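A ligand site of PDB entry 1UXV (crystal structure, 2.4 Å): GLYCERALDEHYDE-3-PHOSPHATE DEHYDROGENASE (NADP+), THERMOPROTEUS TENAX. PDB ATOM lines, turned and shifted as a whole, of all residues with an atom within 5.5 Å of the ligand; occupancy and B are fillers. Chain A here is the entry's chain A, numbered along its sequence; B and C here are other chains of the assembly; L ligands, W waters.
A nitrogen (N4) of the ligand sits close to the backbone carbonyl oxygen (O) of Lys 132 (3.2 Å).
Residues that only touch the ligand: Tyr 184, Arg 155, Gly 135, Ile 133, Glu 156, Pro 139 of chain C, Pro 157 and Val 479.
Hydrophobic or aromatic side chains within 4 Å of the ligand: Ile 133, Pro 157, Tyr 184, Val 479, Pro 139 of chain C, Trp 142 of chain C and Trp 498 of chain C.
Of the 24 residues printed, 17 come within 4 Å of the ligand.
Water W2 lies within hydrogen-bond range of the guanidinium group of Arg 154 (2.5 Å), an oxygen (O2) of the ligand (2.6 Å) and the side-chain hydroxyl of Tyr 137 of chain C (2.7 Å).
Water W1 lies within hydrogen-bond range of an oxygen (O1) of the ligand (2.7 Å), the backbone carbonyl oxygen (O) of Arg 72 (3.0 Å) and the chain-end carboxylate (O) of Glu 501 of chain C (3.4 Å).
Water W3 lies within hydrogen-bond range of the guanidinium group (NH2) of Arg 436 of chain B (2.8 Å) and an oxygen (O2) of the ligand (3.1 Å).
An oxygen (O2) of the ligand is in salt-bridge range of the guanidinium group (NH2) of Arg 154.
NH2 of Arg 72 is in salt-bridge range of O3 of the ligand (2.5 Å).
OD2 of Asp 141 of chain C lies within hydrogen-bond range of O6 of the ligand, 2.9 Å away.
N of Gly 134 lies close to N3 of the ligand (2.7 Å).
An oxygen (O2) of the ligand sits at hydrogen-bond distance from the indole nitrogen of Trp 498 of chain C (3.2 Å).
The indole nitrogen of Trp 142 of chain C is in hydrogen-bond range of an oxygen (O7) of the ligand, at 3.1 Å.
The guanidinium group of Arg 79 lies within hydrogen-bond range of an oxygen (O6) of the ligand, 2.5 Å away.
NE of Arg 440 of chain B is in salt-bridge range of O1 of the ligand (2.4 Å).
NH2 of Arg 72 lies within hydrogen-bond range of O of Arg 440 of chain B.
The side-chain carboxylate (OE2) of Glu 156 lies within salt-bridge range of the guanidinium group (NH2) of Arg 72, 3.4 Å away.
O of Gly 135 sits at hydrogen-bond distance from N of Tyr 137 of chain C (3.2 Å).
O of Glu 156 is in hydrogen-bond range of OG1 of Thr 483, at 3.2 Å.
NE of Arg 79 lies within hydrogen-bond range of O of Met 74 (3.2 Å).
NH2 of Arg 440 of chain B is in salt-bridge range of OD1 of Asp 73, 2.6 Å away.
The side-chain carboxylate (OD2) of Asp 141 of chain C is in salt-bridge range of the guanidinium group (NH2) of Arg 79, at 3.9 Å.
OD2 of Asp 141 of chain C lies within hydrogen-bond range of N of Gly 76, 3.0 Å away.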
ATOM      1  N   ARG A  72      25.805  -3.230  -4.012  1.00  0.00           N
ATOM      2  CA  ARG A  72      24.762  -3.453  -5.009  1.00  0.00           C
ATOM      3  C   ARG A  72      25.093  -2.851  -6.355  1.00  0.00           C
ATOM      4  O   ARG A  72      24.775  -3.430  -7.390  1.00  0.00           O
ATOM      5  CB  ARG A  72      23.412  -2.911  -4.516  1.00  0.00           C
ATOM      6  CG  ARG A  72      22.221  -3.216  -5.428  1.00  0.00           C
ATOM      7  CD  ARG A  72      20.907  -2.721  -4.821  1.00  0.00           C
ATOM      8  NE  ARG A  72      19.750  -2.847  -5.717  1.00  0.00           N
ATOM      9  CZ  ARG A  72      18.536  -2.366  -5.450  1.00  0.00           C
ATOM     10  NH1 ARG A  72      18.299  -1.717  -4.318  1.00  0.00           N
ATOM     11  NH2 ARG A  72      17.551  -2.537  -6.318  1.00  0.00           N
ATOM     12  N   ASP A  73      25.748  -1.689  -6.339  1.00  0.00           N
ATOM     13  CA  ASP A  73      26.072  -1.034  -7.595  1.00  0.00           C
ATOM     14  C   ASP A  73      27.376  -1.491  -8.240  1.00  0.00           C
ATOM     15  O   ASP A  73      27.786  -0.944  -9.257  1.00  0.00           O
ATOM     16  CB  ASP A  73      26.023   0.501  -7.450  1.00  0.00           C
ATOM     17  CG  ASP A  73      24.574   1.031  -7.332  1.00  0.00           C
ATOM     18  OD1 ASP A  73      23.667   0.435  -7.952  1.00  0.00           O
ATOM     19  OD2 ASP A  73      24.331   2.042  -6.638  1.00  0.00           O
ATOM     20  N   MET A  74      28.017  -2.490  -7.652  1.00  0.00           N
ATOM     21  CA  MET A  74      29.203  -3.050  -8.284  1.00  0.00           C
ATOM     22  C   MET A  74      28.616  -4.185  -9.127  1.00  0.00           C
ATOM     23  O   MET A  74      27.989  -5.091  -8.594  1.00  0.00           O
ATOM     24  CB  MET A  74      30.195  -3.619  -7.257  1.00  0.00           C
ATOM     25  CG  MET A  74      31.379  -4.301  -7.921  1.00  0.00           C
ATOM     26  SD  MET A  74      32.632  -4.967  -6.802  1.00  0.00           S
ATOM     27  CE  MET A  74      33.664  -3.451  -6.480  1.00  0.00           C
ATOM     28  N   GLY A  76      27.887  -7.631 -10.938  1.00  0.00           N
ATOM     29  CA  GLY A  76      28.221  -8.977 -10.511  1.00  0.00           C
ATOM     30  C   GLY A  76      29.538  -9.485 -11.066  1.00  0.00           C
ATOM     31  O   GLY A  76      30.301 -10.133 -10.356  1.00  0.00           O
ATOM     32  N   ARG A  79      32.023  -8.150  -8.874  1.00  0.00           N
ATOM     33  CA  ARG A  79      31.992  -8.721  -7.536  1.00  0.00           C
ATOM     34  C   ARG A  79      32.675 -10.087  -7.514  1.00  0.00           C
ATOM     35  O   ARG A  79      33.422 -10.401  -6.605  1.00  0.00           O
ATOM     36  CB  ARG A  79      30.547  -8.847  -7.031  1.00  0.00           C
ATOM     37  CG  ARG A  79      29.944  -7.565  -6.480  1.00  0.00           C
ATOM     38  CD  ARG A  79      28.685  -7.844  -5.632  1.00  0.00           C
ATOM     39  NE  ARG A  79      27.512  -7.363  -6.332  1.00  0.00           N
ATOM     40  CZ  ARG A  79      26.591  -8.135  -6.886  1.00  0.00           C
ATOM     41  NH1 ARG A  79      26.670  -9.444  -6.829  1.00  0.00           N
ATOM     42  NH2 ARG A  79      25.592  -7.574  -7.550  1.00  0.00           N
ATOM     43  N   LYS A 132      21.592 -19.682  -8.795  1.00  0.00           N
ATOM     44  CA  LYS A 132      20.408 -19.164  -8.129  1.00  0.00           C
ATOM     45  C   LYS A 132      20.058 -17.712  -8.471  1.00  0.00           C
ATOM     46  O   LYS A 132      19.281 -17.068  -7.773  1.00  0.00           O
ATOM     47  CB  LYS A 132      20.536 -19.342  -6.610  1.00  0.00           C
ATOM     48  CG  LYS A 132      19.719 -20.504  -6.047  1.00  0.00           C
ATOM     49  CD  LYS A 132      19.889 -21.771  -6.878  1.00  0.00           C
ATOM     50  CE  LYS A 132      19.204 -22.992  -6.213  1.00  0.00           C
ATOM     51  NZ  LYS A 132      17.702 -22.876  -6.080  1.00  0.00           N
ATOM     52  N   ILE A 133      20.650 -17.193  -9.540  1.00  0.00           N
ATOM     53  CA  ILE A 133      20.350 -15.838  -9.997  1.00  0.00           C
ATOM     54  C   ILE A 133      19.324 -16.007 -11.126  1.00  0.00           C
ATOM     55  O   ILE A 133      19.503 -16.869 -11.995  1.00  0.00           O
ATOM     56  CB  ILE A 133      21.616 -15.108 -10.554  1.00  0.00           C
ATOM     57  CG1 ILE A 133      22.197 -14.176  -9.491  1.00  0.00           C
ATOM     58  CG2 ILE A 133      21.261 -14.258 -11.767  1.00  0.00           C
ATOM     59  CD1 ILE A 133      23.447 -14.697  -8.890  1.00  0.00           C
ATOM     60  N   GLY A 134      18.261 -15.201 -11.091  1.00  0.00           N
ATOM     61  CA  GLY A 134      17.240 -15.236 -12.129  1.00  0.00           C
ATOM     62  C   GLY A 134      15.802 -15.585 -11.759  1.00  0.00           C
ATOM     63  O   GLY A 134      15.432 -16.754 -11.665  1.00  0.00           O
ATOM     64  N   GLY A 135      14.984 -14.550 -11.574  1.00  0.00           N
ATOM     65  CA  GLY A 135      13.589 -14.739 -11.214  1.00  0.00           C
ATOM     66  C   GLY A 135      12.595 -15.591 -12.017  1.00  0.00           C
ATOM     67  O   GLY A 135      12.954 -16.380 -12.904  1.00  0.00           O
ATOM     68  N   ARG A 154      11.709 -11.492  -8.678  1.00  0.00           N
ATOM     69  CA  ARG A 154      13.168 -11.576  -8.726  1.00  0.00           C
ATOM     70  C   ARG A 154      13.681 -11.312  -7.316  1.00  0.00           C
ATOM     71  O   ARG A 154      12.978 -10.756  -6.495  1.00  0.00           O
ATOM     72  CB  ARG A 154      13.717 -10.510  -9.683  1.00  0.00           C
ATOM     73  CG  ARG A 154      13.891  -9.172  -8.986  1.00  0.00           C
ATOM     74  CD  ARG A 154      14.162  -7.991  -9.918  1.00  0.00           C
ATOM     75  NE  ARG A 154      15.482  -7.996 -10.538  1.00  0.00           N
ATOM     76  CZ  ARG A 154      16.621  -8.123  -9.866  1.00  0.00           C
ATOM     77  NH1 ARG A 154      16.600  -8.275  -8.558  1.00  0.00           N
ATOM     78  NH2 ARG A 154      17.775  -8.094 -10.520  1.00  0.00           N
ATOM     79  N   ARG A 155      14.927 -11.704  -7.043  1.00  0.00           N
ATOM     80  CA  ARG A 155      15.503 -11.457  -5.722  1.00  0.00           C
ATOM     81  C   ARG A 155      16.408 -10.243  -5.678  1.00  0.00           C
ATOM     82  O   ARG A 155      17.049  -9.900  -6.667  1.00  0.00           O
ATOM     83  CB  ARG A 155      16.258 -12.676  -5.242  1.00  0.00           C
ATOM     84  CG  ARG A 155      15.342 -13.830  -4.999  1.00  0.00           C
ATOM     85  CD  ARG A 155      16.057 -15.018  -4.467  1.00  0.00           C
ATOM     86  NE  ARG A 155      15.466 -15.415  -3.189  1.00  0.00           N
ATOM     87  CZ  ARG A 155      15.125 -16.653  -2.921  1.00  0.00           C
ATOM     88  NH1 ARG A 155      15.317 -17.589  -3.849  1.00  0.00           N
ATOM     89  NH2 ARG A 155      14.594 -16.964  -1.746  1.00  0.00           N
ATOM     90  N   GLU A 156      16.447  -9.593  -4.527  1.00  0.00           N
ATOM     91  CA  GLU A 156      17.305  -8.435  -4.309  1.00  0.00           C
ATOM     92  C   GLU A 156      18.041  -8.648  -3.004  1.00  0.00           C
ATOM     93  O   GLU A 156      17.579  -9.383  -2.130  1.00  0.00           O
ATOM     94  CB  GLU A 156      16.497  -7.147  -4.128  1.00  0.00           C
ATOM     95  CG  GLU A 156      15.657  -6.736  -5.302  1.00  0.00           C
ATOM     96  CD  GLU A 156      15.243  -5.277  -5.199  1.00  0.00           C
ATOM     97  OE1 GLU A 156      15.191  -4.724  -4.068  1.00  0.00           O
ATOM     98  OE2 GLU A 156      14.974  -4.688  -6.257  1.00  0.00           O
ATOM     99  N   PRO A 157      19.240  -8.047  -2.863  1.00  0.00           N
ATOM    100  CA  PRO A 157      19.963  -8.226  -1.609  1.00  0.00           C
ATOM    101  C   PRO A 157      19.160  -7.495  -0.543  1.00  0.00           C
ATOM    102  O   PRO A 157      18.522  -6.489  -0.824  1.00  0.00           O
ATOM    103  CB  PRO A 157      21.311  -7.551  -1.869  1.00  0.00           C
ATOM    104  CG  PRO A 157      21.006  -6.581  -2.998  1.00  0.00           C
ATOM    105  CD  PRO A 157      20.085  -7.376  -3.877  1.00  0.00           C
ATOM    106  N   TYR A 184      25.666 -11.836  -3.939  1.00  0.00           N
ATOM    107  CA  TYR A 184      24.312 -11.382  -4.267  1.00  0.00           C
ATOM    108  C   TYR A 184      24.116  -9.867  -4.074  1.00  0.00           C
ATOM    109  O   TYR A 184      23.021  -9.355  -4.275  1.00  0.00           O
ATOM    110  CB  TYR A 184      23.257 -12.186  -3.464  1.00  0.00           C
ATOM    111  CG  TYR A 184      23.249 -13.685  -3.769  1.00  0.00           C
ATOM    112  CD1 TYR A 184      23.041 -14.146  -5.062  1.00  0.00           C
ATOM    113  CD2 TYR A 184      23.522 -14.640  -2.781  1.00  0.00           C
ATOM    114  CE1 TYR A 184      23.102 -15.498  -5.371  1.00  0.00           C
ATOM    115  CE2 TYR A 184      23.579 -16.014  -3.087  1.00  0.00           C
ATOM    116  CZ  TYR A 184      23.378 -16.431  -4.386  1.00  0.00           C
ATOM    117  OH  TYR A 184      23.459 -17.791  -4.729  1.00  0.00           O
ATOM    118  N   VAL A 479      21.315 -18.293  -0.854  1.00  0.00           N
ATOM    119  CA  VAL A 479      20.649 -17.098  -1.371  1.00  0.00           C
ATOM    120  C   VAL A 479      19.392 -16.741  -0.558  1.00  0.00           C
ATOM    121  O   VAL A 479      19.015 -15.576  -0.415  1.00  0.00           O
ATOM    122  CB  VAL A 479      20.241 -17.306  -2.850  1.00  0.00           C
ATOM    123  CG1 VAL A 479      19.061 -18.255  -2.937  1.00  0.00           C
ATOM    124  CG2 VAL A 479      19.917 -15.976  -3.504  1.00  0.00           C
ATOM    125  N   THR A 483      18.844 -12.694   0.831  1.00  0.00           N
ATOM    126  CA  THR A 483      18.147 -12.073  -0.260  1.00  0.00           C
ATOM    127  C   THR A 483      16.628 -12.010   0.006  1.00  0.00           C
ATOM    128  O   THR A 483      16.120 -12.753   0.832  1.00  0.00           O
ATOM    129  CB  THR A 483      18.524 -12.867  -1.524  1.00  0.00           C
ATOM    130  OG1 THR A 483      19.275 -12.033  -2.418  1.00  0.00           O
ATOM    131  CG2 THR A 483      17.348 -13.476  -2.170  1.00  0.00           C
ATOM    132  N   ARG B 436      10.933   1.231 -15.193  1.00  0.00           N
ATOM    133  CA  ARG B 436      12.053   0.390 -14.773  1.00  0.00           C
ATOM    134  C   ARG B 436      12.808   0.998 -13.606  1.00  0.00           C
ATOM    135  O   ARG B 436      13.107   0.306 -12.639  1.00  0.00           O
ATOM    136  CB  ARG B 436      13.013   0.168 -15.932  1.00  0.00           C
ATOM    137  CG  ARG B 436      14.039  -0.913 -15.619  1.00  0.00           C
ATOM    138  CD  ARG B 436      13.349  -2.251 -15.380  1.00  0.00           C
ATOM    139  NE  ARG B 436      14.254  -3.275 -14.891  1.00  0.00           N
ATOM    140  CZ  ARG B 436      14.691  -3.343 -13.641  1.00  0.00           C
ATOM    141  NH1 ARG B 436      14.297  -2.451 -12.750  1.00  0.00           N
ATOM    142  NH2 ARG B 436      15.486  -4.326 -13.261  1.00  0.00           N
ATOM    143  N   ARG B 440      13.203  -0.645  -9.819  1.00  0.00           N
ATOM    144  CA  ARG B 440      14.474  -0.949  -9.184  1.00  0.00           C
ATOM    145  C   ARG B 440      14.658  -0.260  -7.850  1.00  0.00           C
ATOM    146  O   ARG B 440      15.092  -0.883  -6.878  1.00  0.00           O
ATOM    147  CB  ARG B 440      15.634  -0.558 -10.104  1.00  0.00           C
ATOM    148  CG  ARG B 440      16.978  -0.650  -9.391  1.00  0.00           C
ATOM    149  CD  ARG B 440      18.157  -0.579 -10.358  1.00  0.00           C
ATOM    150  NE  ARG B 440      19.366  -0.829  -9.594  1.00  0.00           N
ATOM    151  CZ  ARG B 440      20.173   0.102  -9.095  1.00  0.00           C
ATOM    152  NH1 ARG B 440      19.917   1.392  -9.288  1.00  0.00           N
ATOM    153  NH2 ARG B 440      21.199  -0.265  -8.342  1.00  0.00           N
ATOM    154  N   TYR C 137      13.929 -14.947 -15.607  1.00  0.00           N
ATOM    155  CA  TYR C 137      14.446 -13.591 -15.680  1.00  0.00           C
ATOM    156  C   TYR C 137      15.970 -13.715 -15.704  1.00  0.00           C
ATOM    157  O   TYR C 137      16.540 -14.508 -14.957  1.00  0.00           O
ATOM    158  CB  TYR C 137      14.022 -12.780 -14.458  1.00  0.00           C
ATOM    159  CG  TYR C 137      14.754 -11.457 -14.328  1.00  0.00           C
ATOM    160  CD1 TYR C 137      14.705 -10.512 -15.348  1.00  0.00           C
ATOM    161  CD2 TYR C 137      15.510 -11.169 -13.195  1.00  0.00           C
ATOM    162  CE1 TYR C 137      15.390  -9.299 -15.244  1.00  0.00           C
ATOM    163  CE2 TYR C 137      16.190  -9.970 -13.067  1.00  0.00           C
ATOM    164  CZ  TYR C 137      16.133  -9.028 -14.091  1.00  0.00           C
ATOM    165  OH  TYR C 137      16.835  -7.848 -13.969  1.00  0.00           O
ATOM    166  N   PRO C 139      19.178 -11.273 -15.333  1.00  0.00           N
ATOM    167  CA  PRO C 139      19.792  -9.953 -15.129  1.00  0.00           C
ATOM    168  C   PRO C 139      21.079  -9.915 -15.966  1.00  0.00           C
ATOM    169  O   PRO C 139      21.748 -10.943 -16.146  1.00  0.00           O
ATOM    170  CB  PRO C 139      20.039  -9.929 -13.621  1.00  0.00           C
ATOM    171  CG  PRO C 139      20.386 -11.335 -13.361  1.00  0.00           C
ATOM    172  CD  PRO C 139      19.367 -12.120 -14.147  1.00  0.00           C
ATOM    173  N   ASP C 141      24.098  -7.984 -15.508  1.00  0.00           N
ATOM    174  CA  ASP C 141      25.397  -7.577 -14.957  1.00  0.00           C
ATOM    175  C   ASP C 141      26.405  -8.658 -14.632  1.00  0.00           C
ATOM    176  O   ASP C 141      27.244  -8.457 -13.761  1.00  0.00           O
ATOM    177  CB  ASP C 141      25.189  -6.706 -13.693  1.00  0.00           C
ATOM    178  CG  ASP C 141      24.474  -7.466 -12.595  1.00  0.00           C
ATOM    179  OD1 ASP C 141      23.431  -8.052 -12.920  1.00  0.00           O
ATOM    180  OD2 ASP C 141      24.944  -7.467 -11.423  1.00  0.00           O
ATOM    181  N   TRP C 142      26.341  -9.806 -15.308  1.00  0.00           N
ATOM    182  CA  TRP C 142      27.305 -10.863 -15.037  1.00  0.00           C
ATOM    183  C   TRP C 142      28.312 -10.975 -16.169  1.00  0.00           C
ATOM    184  O   TRP C 142      29.103 -11.894 -16.231  1.00  0.00           O
ATOM    185  CB  TRP C 142      26.595 -12.194 -14.763  1.00  0.00           C
ATOM    186  CG  TRP C 142      25.805 -12.089 -13.503  1.00  0.00           C
ATOM    187  CD1 TRP C 142      24.487 -11.754 -13.381  1.00  0.00           C
ATOM    188  CD2 TRP C 142      26.328 -12.092 -12.169  1.00  0.00           C
ATOM    189  NE1 TRP C 142      24.165 -11.529 -12.062  1.00  0.00           N
ATOM    190  CE2 TRP C 142      25.282 -11.728 -11.305  1.00  0.00           C
ATOM    191  CE3 TRP C 142      27.603 -12.363 -11.622  1.00  0.00           C
ATOM    192  CZ2 TRP C 142      25.466 -11.621  -9.912  1.00  0.00           C
ATOM    193  CZ3 TRP C 142      27.772 -12.255 -10.249  1.00  0.00           C
ATOM    194  CH2 TRP C 142      26.715 -11.884  -9.416  1.00  0.00           C
ATOM    195  N   TRP C 498      20.518   1.778 -13.768  1.00  0.00           N
ATOM    196  CA  TRP C 498      21.647   1.349 -12.928  1.00  0.00           C
ATOM    197  C   TRP C 498      22.754   2.400 -12.930  1.00  0.00           C
ATOM    198  O   TRP C 498      22.893   3.166 -13.882  1.00  0.00           O
ATOM    199  CB  TRP C 498      22.219   0.025 -13.452  1.00  0.00           C
ATOM    200  CG  TRP C 498      21.283  -1.107 -13.285  1.00  0.00           C
ATOM    201  CD1 TRP C 498      21.013  -1.783 -12.122  1.00  0.00           C
ATOM    202  CD2 TRP C 498      20.434  -1.664 -14.281  1.00  0.00           C
ATOM    203  NE1 TRP C 498      20.043  -2.730 -12.346  1.00  0.00           N
ATOM    204  CE2 TRP C 498      19.668  -2.672 -13.665  1.00  0.00           C
ATOM    205  CE3 TRP C 498      20.242  -1.401 -15.645  1.00  0.00           C
ATOM    206  CZ2 TRP C 498      18.721  -3.426 -14.356  1.00  0.00           C
ATOM    207  CZ3 TRP C 498      19.301  -2.142 -16.336  1.00  0.00           C
ATOM    208  CH2 TRP C 498      18.543  -3.148 -15.691  1.00  0.00           C
ATOM    209  N   GLU C 501      26.504  -0.838 -13.229  1.00  0.00           N
ATOM    210  CA  GLU C 501      26.232  -2.185 -12.684  1.00  0.00           C
ATOM    211  C   GLU C 501      24.956  -2.797 -13.269  1.00  0.00           C
ATOM    212  O   GLU C 501      24.210  -3.492 -12.534  1.00  0.00           O
ATOM    213  CB  GLU C 501      26.095  -2.136 -11.170  1.00  0.00           C
ATOM    214  OXT GLU C 501      24.732  -2.582 -14.476  1.00  0.00           O
HETATM  215  P1  LIG L   1      19.375  -4.354  -9.044  1.00  0.00           P
HETATM  216  O1  LIG L   1      20.079  -3.084  -9.153  1.00  0.00           O
HETATM  217  O2  LIG L   1      19.051  -4.965 -10.335  1.00  0.00           O
HETATM  218  O3  LIG L   1      18.104  -4.192  -8.125  1.00  0.00           O
HETATM  219  O4  LIG L   1      20.370  -5.280  -8.265  1.00  0.00           O
HETATM  220  C1  LIG L   1      19.907  -6.565  -7.952  1.00  0.00           C
HETATM  221  C2  LIG L   1      21.165  -7.326  -7.764  1.00  0.00           C
HETATM  222  O5  LIG L   1      20.669  -8.659  -7.436  1.00  0.00           O
HETATM  223  C3  LIG L   1      22.035  -7.389  -9.200  1.00  0.00           C
HETATM  224  O6  LIG L   1      23.513  -7.416  -8.873  1.00  0.00           O
HETATM  225  C4  LIG L   1      21.419  -8.721  -9.757  1.00  0.00           C
HETATM  226  O7  LIG L   1      22.225  -9.510 -10.654  1.00  0.00           O
HETATM  227  C5  LIG L   1      21.083  -9.564  -8.406  1.00  0.00           C
HETATM  228  N1  LIG L   1      20.032 -10.557  -8.668  1.00  0.00           N
HETATM  229  C6  LIG L   1      19.089 -10.574  -9.712  1.00  0.00           C
HETATM  230  N2  LIG L   1      18.250 -11.608  -9.758  1.00  0.00           N
HETATM  231  C7  LIG L   1      18.722 -12.303  -8.653  1.00  0.00           C
HETATM  232  C8  LIG L   1      18.290 -13.512  -8.126  1.00  0.00           C
HETATM  233  N3  LIG L   1      17.245 -14.166  -8.779  1.00  0.00           N
HETATM  234  N4  LIG L   1      18.979 -13.951  -6.986  1.00  0.00           N
HETATM  235  C9  LIG L   1      19.984 -13.250  -6.415  1.00  0.00           C
HETATM  236  N5  LIG L   1      20.460 -12.066  -6.863  1.00  0.00           N
HETATM  237  C10 LIG L   1      19.794 -11.663  -7.969  1.00  0.00           C
HETATM  238  O   HOH W   1      22.699  -3.262  -9.540  1.00  0.00           O
HETATM  239  O   HOH W   2      18.499  -6.582 -12.313  1.00  0.00           O
HETATM  240  O   HOH W   3      16.227  -3.789 -10.576  1.00  0.00           O
